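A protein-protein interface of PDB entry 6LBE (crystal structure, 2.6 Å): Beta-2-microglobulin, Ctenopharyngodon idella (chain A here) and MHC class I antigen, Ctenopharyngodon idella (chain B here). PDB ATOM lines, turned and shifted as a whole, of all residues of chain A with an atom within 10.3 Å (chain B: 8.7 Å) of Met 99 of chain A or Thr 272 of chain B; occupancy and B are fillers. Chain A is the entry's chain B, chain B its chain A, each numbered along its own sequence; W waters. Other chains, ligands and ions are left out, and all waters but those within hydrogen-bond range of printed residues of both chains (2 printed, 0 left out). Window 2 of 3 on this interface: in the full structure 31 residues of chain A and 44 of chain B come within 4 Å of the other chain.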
ATOM      1  N   SER A  12       2.476 -19.906 -13.500  1.00  0.00           N
ATOM      2  CA  SER A  12       2.136 -19.720 -14.899  1.00  0.00           C
ATOM      3  C   SER A  12       3.374 -19.323 -15.691  1.00  0.00           C
ATOM      4  O   SER A  12       4.316 -18.735 -15.154  1.00  0.00           O
ATOM      5  CB  SER A  12       1.049 -18.661 -15.050  1.00  0.00           C
ATOM      6  OG  SER A  12       1.226 -17.601 -14.126  1.00  0.00           O
ATOM      7  N   ARG A  13       3.385 -19.682 -16.974  1.00  0.00           N
ATOM      8  CA  ARG A  13       4.522 -19.324 -17.816  1.00  0.00           C
ATOM      9  C   ARG A  13       4.691 -17.805 -17.886  1.00  0.00           C
ATOM     10  O   ARG A  13       5.768 -17.272 -17.601  1.00  0.00           O
ATOM     11  CB  ARG A  13       4.345 -19.907 -19.212  1.00  0.00           C
ATOM     12  CG  ARG A  13       5.400 -19.437 -20.171  1.00  0.00           C
ATOM     13  CD  ARG A  13       4.989 -19.666 -21.600  1.00  0.00           C
ATOM     14  NE  ARG A  13       6.146 -19.875 -22.463  1.00  0.00           N
ATOM     15  CZ  ARG A  13       6.966 -18.905 -22.849  1.00  0.00           C
ATOM     16  NH1 ARG A  13       6.742 -17.666 -22.445  1.00  0.00           N
ATOM     17  NH2 ARG A  13       8.005 -19.169 -23.640  1.00  0.00           N
ATOM     18  N   ASN A  14       3.640 -17.096 -18.259  1.00  0.00           N
ATOM     19  CA  ASN A  14       3.559 -15.648 -18.232  1.00  0.00           C
ATOM     20  C   ASN A  14       2.839 -15.169 -16.973  1.00  0.00           C
ATOM     21  O   ASN A  14       2.110 -15.936 -16.331  1.00  0.00           O
ATOM     22  CB  ASN A  14       2.816 -15.147 -19.471  1.00  0.00           C
ATOM     23  CG  ASN A  14       3.441 -15.627 -20.756  1.00  0.00           C
ATOM     24  OD1 ASN A  14       4.661 -15.729 -20.865  1.00  0.00           O
ATOM     25  ND2 ASN A  14       2.610 -15.917 -21.739  1.00  0.00           N
ATOM     26  N   PRO A  15       3.023 -13.898 -16.597  1.00  0.00           N
ATOM     27  CA  PRO A  15       2.329 -13.349 -15.421  1.00  0.00           C
ATOM     28  C   PRO A  15       0.829 -13.598 -15.454  1.00  0.00           C
ATOM     29  O   PRO A  15       0.169 -13.453 -16.484  1.00  0.00           O
ATOM     30  CB  PRO A  15       2.645 -11.852 -15.495  1.00  0.00           C
ATOM     31  CG  PRO A  15       3.996 -11.812 -16.142  1.00  0.00           C
ATOM     32  CD  PRO A  15       3.965 -12.919 -17.176  1.00  0.00           C
ATOM     33  N   GLY A  16       0.292 -13.956 -14.300  1.00  0.00           N
ATOM     34  CA  GLY A  16      -1.072 -14.412 -14.217  1.00  0.00           C
ATOM     35  C   GLY A  16      -2.101 -13.335 -14.425  1.00  0.00           C
ATOM     36  O   GLY A  16      -2.880 -13.038 -13.517  1.00  0.00           O
ATOM     37  N   GLU A  17      -2.137 -12.767 -15.626  1.00  0.00           N
ATOM     38  CA  GLU A  17      -3.131 -11.758 -15.970  1.00  0.00           C
ATOM     39  C   GLU A  17      -4.465 -12.411 -16.305  1.00  0.00           C
ATOM     40  O   GLU A  17      -4.522 -13.295 -17.163  1.00  0.00           O
ATOM     41  CB  GLU A  17      -2.643 -10.950 -17.159  1.00  0.00           C
ATOM     42  CG  GLU A  17      -3.106  -9.531 -17.183  1.00  0.00           C
ATOM     43  CD  GLU A  17      -2.771  -8.891 -18.495  1.00  0.00           C
ATOM     44  OE1 GLU A  17      -1.559  -8.790 -18.814  1.00  0.00           O
ATOM     45  OE2 GLU A  17      -3.730  -8.527 -19.217  1.00  0.00           O
ATOM     46  N   TYR A  18      -5.537 -11.959 -15.645  1.00  0.00           N
ATOM     47  CA  TYR A  18      -6.886 -12.448 -15.929  1.00  0.00           C
ATOM     48  C   TYR A  18      -7.276 -12.204 -17.390  1.00  0.00           C
ATOM     49  O   TYR A  18      -7.001 -11.147 -17.967  1.00  0.00           O
ATOM     50  CB  TYR A  18      -7.911 -11.785 -14.987  1.00  0.00           C
ATOM     51  CG  TYR A  18      -7.733 -12.202 -13.545  1.00  0.00           C
ATOM     52  CD1 TYR A  18      -7.345 -13.494 -13.238  1.00  0.00           C
ATOM     53  CD2 TYR A  18      -7.889 -11.309 -12.500  1.00  0.00           C
ATOM     54  CE1 TYR A  18      -7.146 -13.905 -11.950  1.00  0.00           C
ATOM     55  CE2 TYR A  18      -7.689 -11.718 -11.187  1.00  0.00           C
ATOM     56  CZ  TYR A  18      -7.322 -13.025 -10.926  1.00  0.00           C
ATOM     57  OH  TYR A  18      -7.104 -13.487  -9.640  1.00  0.00           O
ATOM     58  N   GLY A  19      -7.948 -13.189 -17.984  1.00  0.00           N
ATOM     59  CA  GLY A  19      -8.416 -13.057 -19.339  1.00  0.00           C
ATOM     60  C   GLY A  19      -7.392 -13.330 -20.422  1.00  0.00           C
ATOM     61  O   GLY A  19      -7.759 -13.319 -21.601  1.00  0.00           O
ATOM     62  N   LYS A  20      -6.133 -13.592 -20.084  1.00  0.00           N
ATOM     63  CA  LYS A  20      -5.098 -13.803 -21.090  1.00  0.00           C
ATOM     64  C   LYS A  20      -4.683 -15.273 -21.113  1.00  0.00           C
ATOM     65  O   LYS A  20      -4.345 -15.843 -20.072  1.00  0.00           O
ATOM     66  CB  LYS A  20      -3.896 -12.893 -20.818  1.00  0.00           C
ATOM     67  CG  LYS A  20      -3.609 -11.853 -21.920  1.00  0.00           C
ATOM     68  CD  LYS A  20      -4.510 -10.596 -21.820  1.00  0.00           C
ATOM     69  CE  LYS A  20      -4.788  -9.949 -23.200  1.00  0.00           C
ATOM     70  NZ  LYS A  20      -5.725  -8.776 -23.117  1.00  0.00           N
ATOM     71  N   ASN A  22      -2.588 -18.547 -21.312  1.00  0.00           N
ATOM     72  CA  ASN A  22      -1.360 -18.713 -20.560  1.00  0.00           C
ATOM     73  C   ASN A  22      -1.134 -20.215 -20.395  1.00  0.00           C
ATOM     74  O   ASN A  22      -1.917 -21.038 -20.889  1.00  0.00           O
ATOM     75  CB  ASN A  22      -1.561 -18.081 -19.177  1.00  0.00           C
ATOM     76  CG  ASN A  22      -0.270 -17.749 -18.487  1.00  0.00           C
ATOM     77  OD1 ASN A  22       0.721 -18.444 -18.648  1.00  0.00           O
ATOM     78  ND2 ASN A  22      -0.279 -16.688 -17.691  1.00  0.00           N
ATOM     79  N   PHE A  71      -4.220 -22.819 -20.095  1.00  0.00           N
ATOM     80  CA  PHE A  71      -5.353 -22.361 -19.310  1.00  0.00           C
ATOM     81  C   PHE A  71      -5.567 -20.882 -19.592  1.00  0.00           C
ATOM     82  O   PHE A  71      -4.742 -20.211 -20.225  1.00  0.00           O
ATOM     83  CB  PHE A  71      -5.173 -22.692 -17.807  1.00  0.00           C
ATOM     84  CG  PHE A  71      -4.331 -21.709 -17.023  1.00  0.00           C
ATOM     85  CD1 PHE A  71      -3.105 -21.247 -17.503  1.00  0.00           C
ATOM     86  CD2 PHE A  71      -4.742 -21.290 -15.764  1.00  0.00           C
ATOM     87  CE1 PHE A  71      -2.313 -20.349 -16.753  1.00  0.00           C
ATOM     88  CE2 PHE A  71      -3.964 -20.402 -15.007  1.00  0.00           C
ATOM     89  CZ  PHE A  71      -2.743 -19.932 -15.510  1.00  0.00           C
ATOM     90  N   PRO A  73      -6.980 -17.819 -17.206  1.00  0.00           N
ATOM     91  CA  PRO A  73      -7.313 -17.661 -15.786  1.00  0.00           C
ATOM     92  C   PRO A  73      -8.331 -16.526 -15.734  1.00  0.00           C
ATOM     93  O   PRO A  73      -8.101 -15.437 -16.261  1.00  0.00           O
ATOM     94  CB  PRO A  73      -6.015 -17.283 -15.070  1.00  0.00           C
ATOM     95  CG  PRO A  73      -5.201 -16.639 -16.149  1.00  0.00           C
ATOM     96  CD  PRO A  73      -5.488 -17.462 -17.385  1.00  0.00           C
ATOM     97  N   PRO A  75     -11.103 -14.470 -12.846  1.00  0.00           N
ATOM     98  CA  PRO A  75     -11.378 -14.293 -11.413  1.00  0.00           C
ATOM     99  C   PRO A  75     -12.349 -15.340 -10.871  1.00  0.00           C
ATOM    100  O   PRO A  75     -13.277 -15.782 -11.552  1.00  0.00           O
ATOM    101  CB  PRO A  75     -11.979 -12.881 -11.348  1.00  0.00           C
ATOM    102  CG  PRO A  75     -11.386 -12.171 -12.565  1.00  0.00           C
ATOM    103  CD  PRO A  75     -11.292 -13.219 -13.617  1.00  0.00           C
ATOM    104  N   TRP A  95      -2.733 -22.515  -7.226  1.00  0.00           N
ATOM    105  CA  TRP A  95      -2.008 -21.514  -7.986  1.00  0.00           C
ATOM    106  C   TRP A  95      -2.394 -20.116  -7.515  1.00  0.00           C
ATOM    107  O   TRP A  95      -3.582 -19.757  -7.481  1.00  0.00           O
ATOM    108  CB  TRP A  95      -2.281 -21.673  -9.469  1.00  0.00           C
ATOM    109  CG  TRP A  95      -1.653 -20.602 -10.308  1.00  0.00           C
ATOM    110  CD1 TRP A  95      -0.321 -20.459 -10.608  1.00  0.00           C
ATOM    111  CD2 TRP A  95      -2.331 -19.525 -10.961  1.00  0.00           C
ATOM    112  NE1 TRP A  95      -0.136 -19.357 -11.406  1.00  0.00           N
ATOM    113  CE2 TRP A  95      -1.353 -18.766 -11.639  1.00  0.00           C
ATOM    114  CE3 TRP A  95      -3.671 -19.129 -11.039  1.00  0.00           C
ATOM    115  CZ2 TRP A  95      -1.677 -17.630 -12.389  1.00  0.00           C
ATOM    116  CZ3 TRP A  95      -3.988 -18.009 -11.774  1.00  0.00           C
ATOM    117  CH2 TRP A  95      -2.994 -17.266 -12.440  1.00  0.00           C
ATOM    118  N   GLU A  96      -1.378 -19.332  -7.136  1.00  0.00           N
ATOM    119  CA  GLU A  96      -1.560 -17.949  -6.749  1.00  0.00           C
ATOM    120  C   GLU A  96      -0.879 -17.038  -7.761  1.00  0.00           C
ATOM    121  O   GLU A  96       0.355 -17.074  -7.886  1.00  0.00           O
ATOM    122  CB  GLU A  96      -0.993 -17.717  -5.353  1.00  0.00           C
ATOM    123  CG  GLU A  96      -1.679 -18.490  -4.264  1.00  0.00           C
ATOM    124  CD  GLU A  96      -3.137 -18.092  -4.072  1.00  0.00           C
ATOM    125  OE1 GLU A  96      -3.594 -17.091  -4.681  1.00  0.00           O
ATOM    126  OE2 GLU A  96      -3.827 -18.794  -3.290  1.00  0.00           O
ATOM    127  N   PRO A  97      -1.621 -16.206  -8.490  1.00  0.00           N
ATOM    128  CA  PRO A  97      -0.971 -15.219  -9.367  1.00  0.00           C
ATOM    129  C   PRO A  97      -0.124 -14.219  -8.586  1.00  0.00           C
ATOM    130  O   PRO A  97      -0.417 -13.868  -7.441  1.00  0.00           O
ATOM    131  CB  PRO A  97      -2.150 -14.525 -10.066  1.00  0.00           C
ATOM    132  CG  PRO A  97      -3.356 -14.852  -9.230  1.00  0.00           C
ATOM    133  CD  PRO A  97      -3.088 -16.179  -8.599  1.00  0.00           C
ATOM    134  N   ASP A  98       0.943 -13.755  -9.227  1.00  0.00           N
ATOM    135  CA  ASP A  98       1.853 -12.802  -8.611  1.00  0.00           C
ATOM    136  C   ASP A  98       1.484 -11.365  -8.936  1.00  0.00           C
ATOM    137  O   ASP A  98       2.204 -10.445  -8.537  1.00  0.00           O
ATOM    138  CB  ASP A  98       3.287 -13.095  -9.043  1.00  0.00           C
ATOM    139  CG  ASP A  98       3.878 -14.265  -8.300  1.00  0.00           C
ATOM    140  OD1 ASP A  98       3.682 -14.359  -7.064  1.00  0.00           O
ATOM    141  OD2 ASP A  98       4.522 -15.100  -8.964  1.00  0.00           O
ATOM    142  N   MET A  99       0.375 -11.164  -9.642  1.00  0.00           N
ATOM    143  CA  MET A  99      -0.168  -9.849  -9.930  1.00  0.00           C
ATOM    144  C   MET A  99      -1.649  -9.816  -9.575  1.00  0.00           C
ATOM    145  O   MET A  99      -2.286 -10.872  -9.519  1.00  0.00           O
ATOM    146  CB  MET A  99       0.031  -9.517 -11.397  1.00  0.00           C
ATOM    147  CG  MET A  99      -0.454 -10.591 -12.345  1.00  0.00           C
ATOM    148  SD  MET A  99      -0.192 -10.048 -14.047  1.00  0.00           S
ATOM    149  CE  MET A  99      -1.300  -8.644 -14.068  1.00  0.00           C
ATOM    150  N   SER B 184       8.507  -8.341 -16.537  1.00  0.00           N
ATOM    151  CA  SER B 184       7.404  -7.540 -16.038  1.00  0.00           C
ATOM    152  C   SER B 184       7.618  -7.225 -14.573  1.00  0.00           C
ATOM    153  O   SER B 184       8.292  -7.966 -13.852  1.00  0.00           O
ATOM    154  CB  SER B 184       6.072  -8.252 -16.203  1.00  0.00           C
ATOM    155  OG  SER B 184       6.046  -8.982 -17.407  1.00  0.00           O
ATOM    156  N   LEU B 185       7.041  -6.111 -14.144  1.00  0.00           N
ATOM    157  CA  LEU B 185       6.968  -5.757 -12.736  1.00  0.00           C
ATOM    158  C   LEU B 185       5.538  -5.980 -12.286  1.00  0.00           C
ATOM    159  O   LEU B 185       4.608  -5.396 -12.851  1.00  0.00           O
ATOM    160  CB  LEU B 185       7.393  -4.311 -12.494  1.00  0.00           C
ATOM    161  CG  LEU B 185       8.862  -4.027 -12.193  1.00  0.00           C
ATOM    162  CD1 LEU B 185       8.985  -2.653 -11.551  1.00  0.00           C
ATOM    163  CD2 LEU B 185       9.457  -5.081 -11.288  1.00  0.00           C
ATOM    164  N   LEU B 186       5.366  -6.823 -11.279  1.00  0.00           N
ATOM    165  CA  LEU B 186       4.051  -7.284 -10.865  1.00  0.00           C
ATOM    166  C   LEU B 186       3.698  -6.742  -9.481  1.00  0.00           C
ATOM    167  O   LEU B 186       4.565  -6.562  -8.616  1.00  0.00           O
ATOM    168  CB  LEU B 186       4.014  -8.815 -10.855  1.00  0.00           C
ATOM    169  CG  LEU B 186       3.755  -9.630 -12.127  1.00  0.00           C
ATOM    170  CD1 LEU B 186       4.424  -9.070 -13.345  1.00  0.00           C
ATOM    171  CD2 LEU B 186       4.205 -11.065 -11.929  1.00  0.00           C
ATOM    172  N   GLN B 187       2.412  -6.498  -9.259  1.00  0.00           N
ATOM    173  CA  GLN B 187       1.966  -6.158  -7.918  1.00  0.00           C
ATOM    174  C   GLN B 187       0.528  -6.608  -7.740  1.00  0.00           C
ATOM    175  O   GLN B 187      -0.322  -6.281  -8.568  1.00  0.00           O
ATOM    176  CB  GLN B 187       2.084  -4.656  -7.670  1.00  0.00           C
ATOM    177  CG  GLN B 187       2.215  -4.261  -6.215  1.00  0.00           C
ATOM    178  CD  GLN B 187       2.410  -2.780  -6.081  1.00  0.00           C
ATOM    179  OE1 GLN B 187       1.774  -2.010  -6.792  1.00  0.00           O
ATOM    180  NE2 GLN B 187       3.305  -2.366  -5.196  1.00  0.00           N
ATOM    181  N   LYS B 188       0.262  -7.339  -6.654  1.00  0.00           N
ATOM    182  CA  LYS B 188      -1.098  -7.804  -6.374  1.00  0.00           C
ATOM    183  C   LYS B 188      -2.022  -6.658  -5.944  1.00  0.00           C
ATOM    184  O   LYS B 188      -3.165  -6.572  -6.412  1.00  0.00           O
ATOM    185  CB  LYS B 188      -1.059  -8.907  -5.310  1.00  0.00           C
ATOM    186  CG  LYS B 188      -0.550 -10.256  -5.829  1.00  0.00           C
ATOM    187  CD  LYS B 188      -0.088 -11.180  -4.700  1.00  0.00           C
ATOM    188  CE  LYS B 188       1.410 -11.003  -4.390  1.00  0.00           C
ATOM    189  NZ  LYS B 188       2.271 -12.212  -4.703  1.00  0.00           N
ATOM    190  N   ASP B 189      -1.562  -5.779  -5.056  1.00  0.00           N
ATOM    191  CA  ASP B 189      -2.368  -4.662  -4.579  1.00  0.00           C
ATOM    192  C   ASP B 189      -1.438  -3.496  -4.271  1.00  0.00           C
ATOM    193  O   ASP B 189      -0.214  -3.674  -4.193  1.00  0.00           O
ATOM    194  CB  ASP B 189      -3.196  -5.058  -3.353  1.00  0.00           C
ATOM    195  CG  ASP B 189      -2.357  -5.637  -2.235  1.00  0.00           C
ATOM    196  OD1 ASP B 189      -1.644  -4.857  -1.565  1.00  0.00           O
ATOM    197  OD2 ASP B 189      -2.424  -6.871  -2.015  1.00  0.00           O
ATOM    198  N   PRO B 190      -1.983  -2.276  -4.116  1.00  0.00           N
ATOM    199  CA  PRO B 190      -1.119  -1.072  -4.093  1.00  0.00           C
ATOM    200  C   PRO B 190      -0.082  -1.038  -2.983  1.00  0.00           C
ATOM    201  O   PRO B 190       0.844  -0.217  -3.061  1.00  0.00           O
ATOM    202  CB  PRO B 190      -2.120   0.076  -3.931  1.00  0.00           C
ATOM    203  CG  PRO B 190      -3.395  -0.448  -4.492  1.00  0.00           C
ATOM    204  CD  PRO B 190      -3.416  -1.911  -4.171  1.00  0.00           C
ATOM    205  N   SER B 191      -0.201  -1.893  -1.964  1.00  0.00           N
ATOM    206  CA  SER B 191       0.740  -1.947  -0.853  1.00  0.00           C
ATOM    207  C   SER B 191       1.617  -3.197  -0.841  1.00  0.00           C
ATOM    208  O   SER B 191       2.631  -3.210  -0.131  1.00  0.00           O
ATOM    209  CB  SER B 191      -0.018  -1.875   0.480  1.00  0.00           C
ATOM    210  OG  SER B 191      -0.536  -3.147   0.816  1.00  0.00           O
ATOM    211  N   SER B 192       1.237  -4.245  -1.589  1.00  0.00           N
ATOM    212  CA  SER B 192       1.953  -5.509  -1.766  1.00  0.00           C
ATOM    213  C   SER B 192       3.421  -5.316  -2.119  1.00  0.00           C
ATOM    214  O   SER B 192       3.791  -4.304  -2.717  1.00  0.00           O
ATOM    215  CB  SER B 192       1.348  -6.309  -2.923  1.00  0.00           C
ATOM    216  OG  SER B 192       0.308  -7.162  -2.493  1.00  0.00           O
ATOM    217  N   PRO B 193       4.284  -6.267  -1.782  1.00  0.00           N
ATOM    218  CA  PRO B 193       5.610  -6.294  -2.403  1.00  0.00           C
ATOM    219  C   PRO B 193       5.516  -6.336  -3.918  1.00  0.00           C
ATOM    220  O   PRO B 193       4.469  -6.655  -4.488  1.00  0.00           O
ATOM    221  CB  PRO B 193       6.268  -7.553  -1.836  1.00  0.00           C
ATOM    222  CG  PRO B 193       5.151  -8.359  -1.259  1.00  0.00           C
ATOM    223  CD  PRO B 193       4.099  -7.412  -0.853  1.00  0.00           C
ATOM    224  N   THR B 195       7.231  -7.546  -7.699  1.00  0.00           N
ATOM    225  CA  THR B 195       7.903  -8.729  -8.215  1.00  0.00           C
ATOM    226  C   THR B 195       8.443  -8.454  -9.603  1.00  0.00           C
ATOM    227  O   THR B 195       7.694  -8.051 -10.501  1.00  0.00           O
ATOM    228  CB  THR B 195       6.956  -9.928  -8.249  1.00  0.00           C
ATOM    229  OG1 THR B 195       6.431 -10.154  -6.931  1.00  0.00           O
ATOM    230  CG2 THR B 195       7.707 -11.155  -8.714  1.00  0.00           C
ATOM    231  N   HIS B 197       9.570 -10.199 -12.758  1.00  0.00           N
ATOM    232  CA  HIS B 197       9.336 -11.511 -13.346  1.00  0.00           C
ATOM    233  C   HIS B 197      10.010 -11.575 -14.704  1.00  0.00           C
ATOM    234  O   HIS B 197       9.794 -10.704 -15.548  1.00  0.00           O
ATOM    235  CB  HIS B 197       7.840 -11.775 -13.474  1.00  0.00           C
ATOM    236  CG  HIS B 197       7.504 -13.105 -14.071  1.00  0.00           C
ATOM    237  ND1 HIS B 197       7.374 -13.304 -15.429  1.00  0.00           N
ATOM    238  CD2 HIS B 197       7.249 -14.303 -13.491  1.00  0.00           C
ATOM    239  CE1 HIS B 197       7.060 -14.568 -15.659  1.00  0.00           C
ATOM    240  NE2 HIS B 197       6.977 -15.196 -14.500  1.00  0.00           N
ATOM    241  N   MET B 237      12.098 -15.221 -10.959  1.00  0.00           N
ATOM    242  CA  MET B 237      11.583 -13.963 -10.454  1.00  0.00           C
ATOM    243  C   MET B 237      12.280 -13.583  -9.152  1.00  0.00           C
ATOM    244  O   MET B 237      12.818 -14.428  -8.436  1.00  0.00           O
ATOM    245  CB  MET B 237      10.061 -14.034 -10.259  1.00  0.00           C
ATOM    246  CG  MET B 237       9.585 -14.925  -9.121  1.00  0.00           C
ATOM    247  SD  MET B 237       7.766 -14.919  -9.046  1.00  0.00           S
ATOM    248  CE  MET B 237       7.473 -15.383  -7.341  1.00  0.00           C
ATOM    249  N   ASP B 269       6.118   0.742 -14.927  1.00  0.00           N
ATOM    250  CA  ASP B 269       5.797  -0.493 -15.627  1.00  0.00           C
ATOM    251  C   ASP B 269       4.853  -1.407 -14.859  1.00  0.00           C
ATOM    252  O   ASP B 269       4.270  -2.303 -15.477  1.00  0.00           O
ATOM    253  CB  ASP B 269       7.077  -1.259 -15.948  1.00  0.00           C
ATOM    254  CG  ASP B 269       8.002  -0.471 -16.846  1.00  0.00           C
ATOM    255  OD1 ASP B 269       7.612  -0.189 -17.998  1.00  0.00           O
ATOM    256  OD2 ASP B 269       9.110  -0.113 -16.404  1.00  0.00           O
ATOM    257  N   ILE B 270       4.664  -1.194 -13.554  1.00  0.00           N
ATOM    258  CA  ILE B 270       3.884  -2.095 -12.702  1.00  0.00           C
ATOM    259  C   ILE B 270       2.525  -2.452 -13.307  1.00  0.00           C
ATOM    260  O   ILE B 270       1.666  -1.582 -13.476  1.00  0.00           O
ATOM    261  CB  ILE B 270       3.685  -1.474 -11.308  1.00  0.00           C
ATOM    262  CG1 ILE B 270       5.010  -1.354 -10.582  1.00  0.00           C
ATOM    263  CG2 ILE B 270       2.716  -2.299 -10.485  1.00  0.00           C
ATOM    264  CD1 ILE B 270       4.873  -0.963  -9.124  1.00  0.00           C
ATOM    265  N   ILE B 271       2.317  -3.732 -13.623  1.00  0.00           N
ATOM    266  CA  ILE B 271       1.005  -4.237 -14.006  1.00  0.00           C
ATOM    267  C   ILE B 271       0.392  -4.992 -12.830  1.00  0.00           C
ATOM    268  O   ILE B 271       1.069  -5.349 -11.861  1.00  0.00           O
ATOM    269  CB  ILE B 271       1.058  -5.122 -15.274  1.00  0.00           C
ATOM    270  CG1 ILE B 271       2.086  -6.243 -15.127  1.00  0.00           C
ATOM    271  CG2 ILE B 271       1.400  -4.298 -16.466  1.00  0.00           C
ATOM    272  CD1 ILE B 271       1.972  -7.331 -16.226  1.00  0.00           C
ATOM    273  N   THR B 272      -0.918  -5.225 -12.910  1.00  0.00           N
ATOM    274  CA  THR B 272      -1.657  -5.716 -11.754  1.00  0.00           C
ATOM    275  C   THR B 272      -3.017  -6.222 -12.198  1.00  0.00           C
ATOM    276  O   THR B 272      -3.575  -5.745 -13.189  1.00  0.00           O
ATOM    277  CB  THR B 272      -1.832  -4.623 -10.687  1.00  0.00           C
ATOM    278  OG1 THR B 272      -2.636  -5.117  -9.605  1.00  0.00           O
ATOM    279  CG2 THR B 272      -2.501  -3.409 -11.271  1.00  0.00           C
ATOM    280  N   ASN B 273      -3.546  -7.188 -11.447  1.00  0.00           N
ATOM    281  CA  ASN B 273      -4.910  -7.647 -11.656  1.00  0.00           C
ATOM    282  C   ASN B 273      -5.910  -6.814 -10.884  1.00  0.00           C
ATOM    283  O   ASN B 273      -7.093  -6.797 -11.243  1.00  0.00           O
ATOM    284  CB  ASN B 273      -5.064  -9.119 -11.241  1.00  0.00           C
ATOM    285  CG  ASN B 273      -4.588 -10.096 -12.317  1.00  0.00           C
ATOM    286  OD1 ASN B 273      -4.673  -9.820 -13.516  1.00  0.00           O
ATOM    287  ND2 ASN B 273      -4.090 -11.247 -11.883  1.00  0.00           N
ATOM    288  N   PHE B 274      -5.460  -6.134  -9.838  1.00  0.00           N
ATOM    289  CA  PHE B 274      -6.303  -5.243  -9.048  1.00  0.00           C
ATOM    290  C   PHE B 274      -6.718  -4.015  -9.851  1.00  0.00           C
ATOM    291  O   PHE B 274      -7.848  -3.929 -10.328  1.00  0.00           O
ATOM    292  CB  PHE B 274      -5.556  -4.819  -7.785  1.00  0.00           C
ATOM    293  CG  PHE B 274      -6.426  -4.171  -6.757  1.00  0.00           C
ATOM    294  CD1 PHE B 274      -7.623  -4.758  -6.372  1.00  0.00           C
ATOM    295  CD2 PHE B 274      -6.046  -2.975  -6.167  1.00  0.00           C
ATOM    296  CE1 PHE B 274      -8.432  -4.157  -5.423  1.00  0.00           C
ATOM    297  CE2 PHE B 274      -6.844  -2.369  -5.220  1.00  0.00           C
ATOM    298  CZ  PHE B 274      -8.040  -2.961  -4.845  1.00  0.00           C
HETATM  299  O   HOH W   1       4.868 -17.084 -12.800  1.00  0.00           O
HETATM  300  O   HOH W   2       3.907 -10.149  -6.404  1.00  0.00           O
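The side-chain amide nitrogen of Asn 273 of chain B is in hydrogen-bond range of the backbone carbonyl oxygen of Met 99 of chain A (3.0 Å). SD of Met 237 of chain B lies close to OD2 of Asp 98 of chain A, 3.3 Å away. The backbone carbonyl oxygen of Gly 16 of chain A lies within hydrogen-bond range of the side-chain amide nitrogen of Asn 273 of chain B (2.7 Å). The side-chain amino group (NZ) of Lys 188 of chain B lies within salt-bridge range of the side-chain carboxylate (OD1) of Asp 98 of chain A (3.5 Å). The backbone NH (N) of Tyr 18 of chain A lies within hydrogen-bond range of the side-chain amide oxygen (OD1) of Asn 273 of chain B (3.1 Å).
ND2 of Asn 22 of chain A sits at hydrogen-bond distance from O of Pro 15 of chain A (3.5 Å). N of Leu 186 of chain B sits at hydrogen-bond distance from O of Thr 195 of chain B (2.7 Å). N of Gln 187 of chain B lies within hydrogen-bond range of O of Ile 271 of chain B (3.1 Å). The backbone NH (N) of Arg 13 of chain A lies within hydrogen-bond range of the side-chain amide oxygen (OD1) of Asn 22 of chain A. The backbone carbonyl oxygen of Ser 184 of chain B lies within hydrogen-bond range of the backbone NH of His 197 of chain B, 2.8 Å away. NE2 of Gln 187 of chain B lies within hydrogen-bond range of O of Ser 192 of chain B, at 3.2 Å.
Among the printed residues, merely in contact across the chains: Arg 13 of chain A with His 197 of chain B, Pro 15 of chain A with Ser 184 of chain B, Pro 15 of chain A with Leu 186 of chain B, Pro 15 of chain A with His 197 of chain B, Glu 17 of chain A with Asn 273 of chain B, Pro 97 of chain A with Lys 188 of chain B, Asp 98 of chain A with Leu 186 of chain B, Met 99 of chain A with Leu 186 of chain B, Met 99 of chain A with Gln 187 of chain B, Met 99 of chain A with Lys 188 of chain B and Met 99 of chain A with Thr 272 of chain B.
Printed residues of chain B within 4 Å of Arg 13 of chain A: His 197 (3.6 Å). Gly 16 of chain A touches one residue of chain B. Of the printed residues of chain B, Asp 98 of chain A touches Leu 186, Lys 188 and Met 237. Met 99 of chain A touches just these residues of chain B: Leu 186 (3.8 Å), Gln 187 (3.8 Å), Lys 188 (3.8 Å), Thr 272 (3.5 Å) and Asn 273 (3.0 Å). Of the printed residues of chain A, Lys 188 of chain B touches Pro 97, Asp 98 and Met 99. Thr 272 of chain B touches just one residue of chain A: Met 99. Asn 273 of chain B touches just these residues of chain A: Gly 16, Glu 17, Tyr 18 and Met 99. The nearest printed residue of chain B that does not touch Pro 97 of chain A is Asn 273 of chain B (4.2 Å).
Of the 18 printed residues of chain A, 8 touch a printed residue of chain B. Printed residues of chain A that touch a printed residue of chain B: Arg 13, Pro 15, Gly 16, Glu 17, Tyr 18, Pro 97, Asp 98 and Met 99. Of the 19 printed residues of chain B, 8 touch a printed residue of chain A. Printed residues of chain B that touch a printed residue of chain A: Ser 184, Leu 186, Gln 187, Lys 188, His 197, Met 237, Thr 272 and Asn 273.
Water W2 lies within hydrogen-bond range of the side-chain hydroxyl of Thr 195 of chain B (2.6 Å), the backbone carbonyl oxygen of Asp 98 of chain A (2.7 Å) and the side-chain amino group of Lys 188 of chain B (3.1 Å). Water W1 bridges the backbone carbonyl oxygen (O) of Ser 12 of chain A and a ring nitrogen (NE2) of His 197 of chain B.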
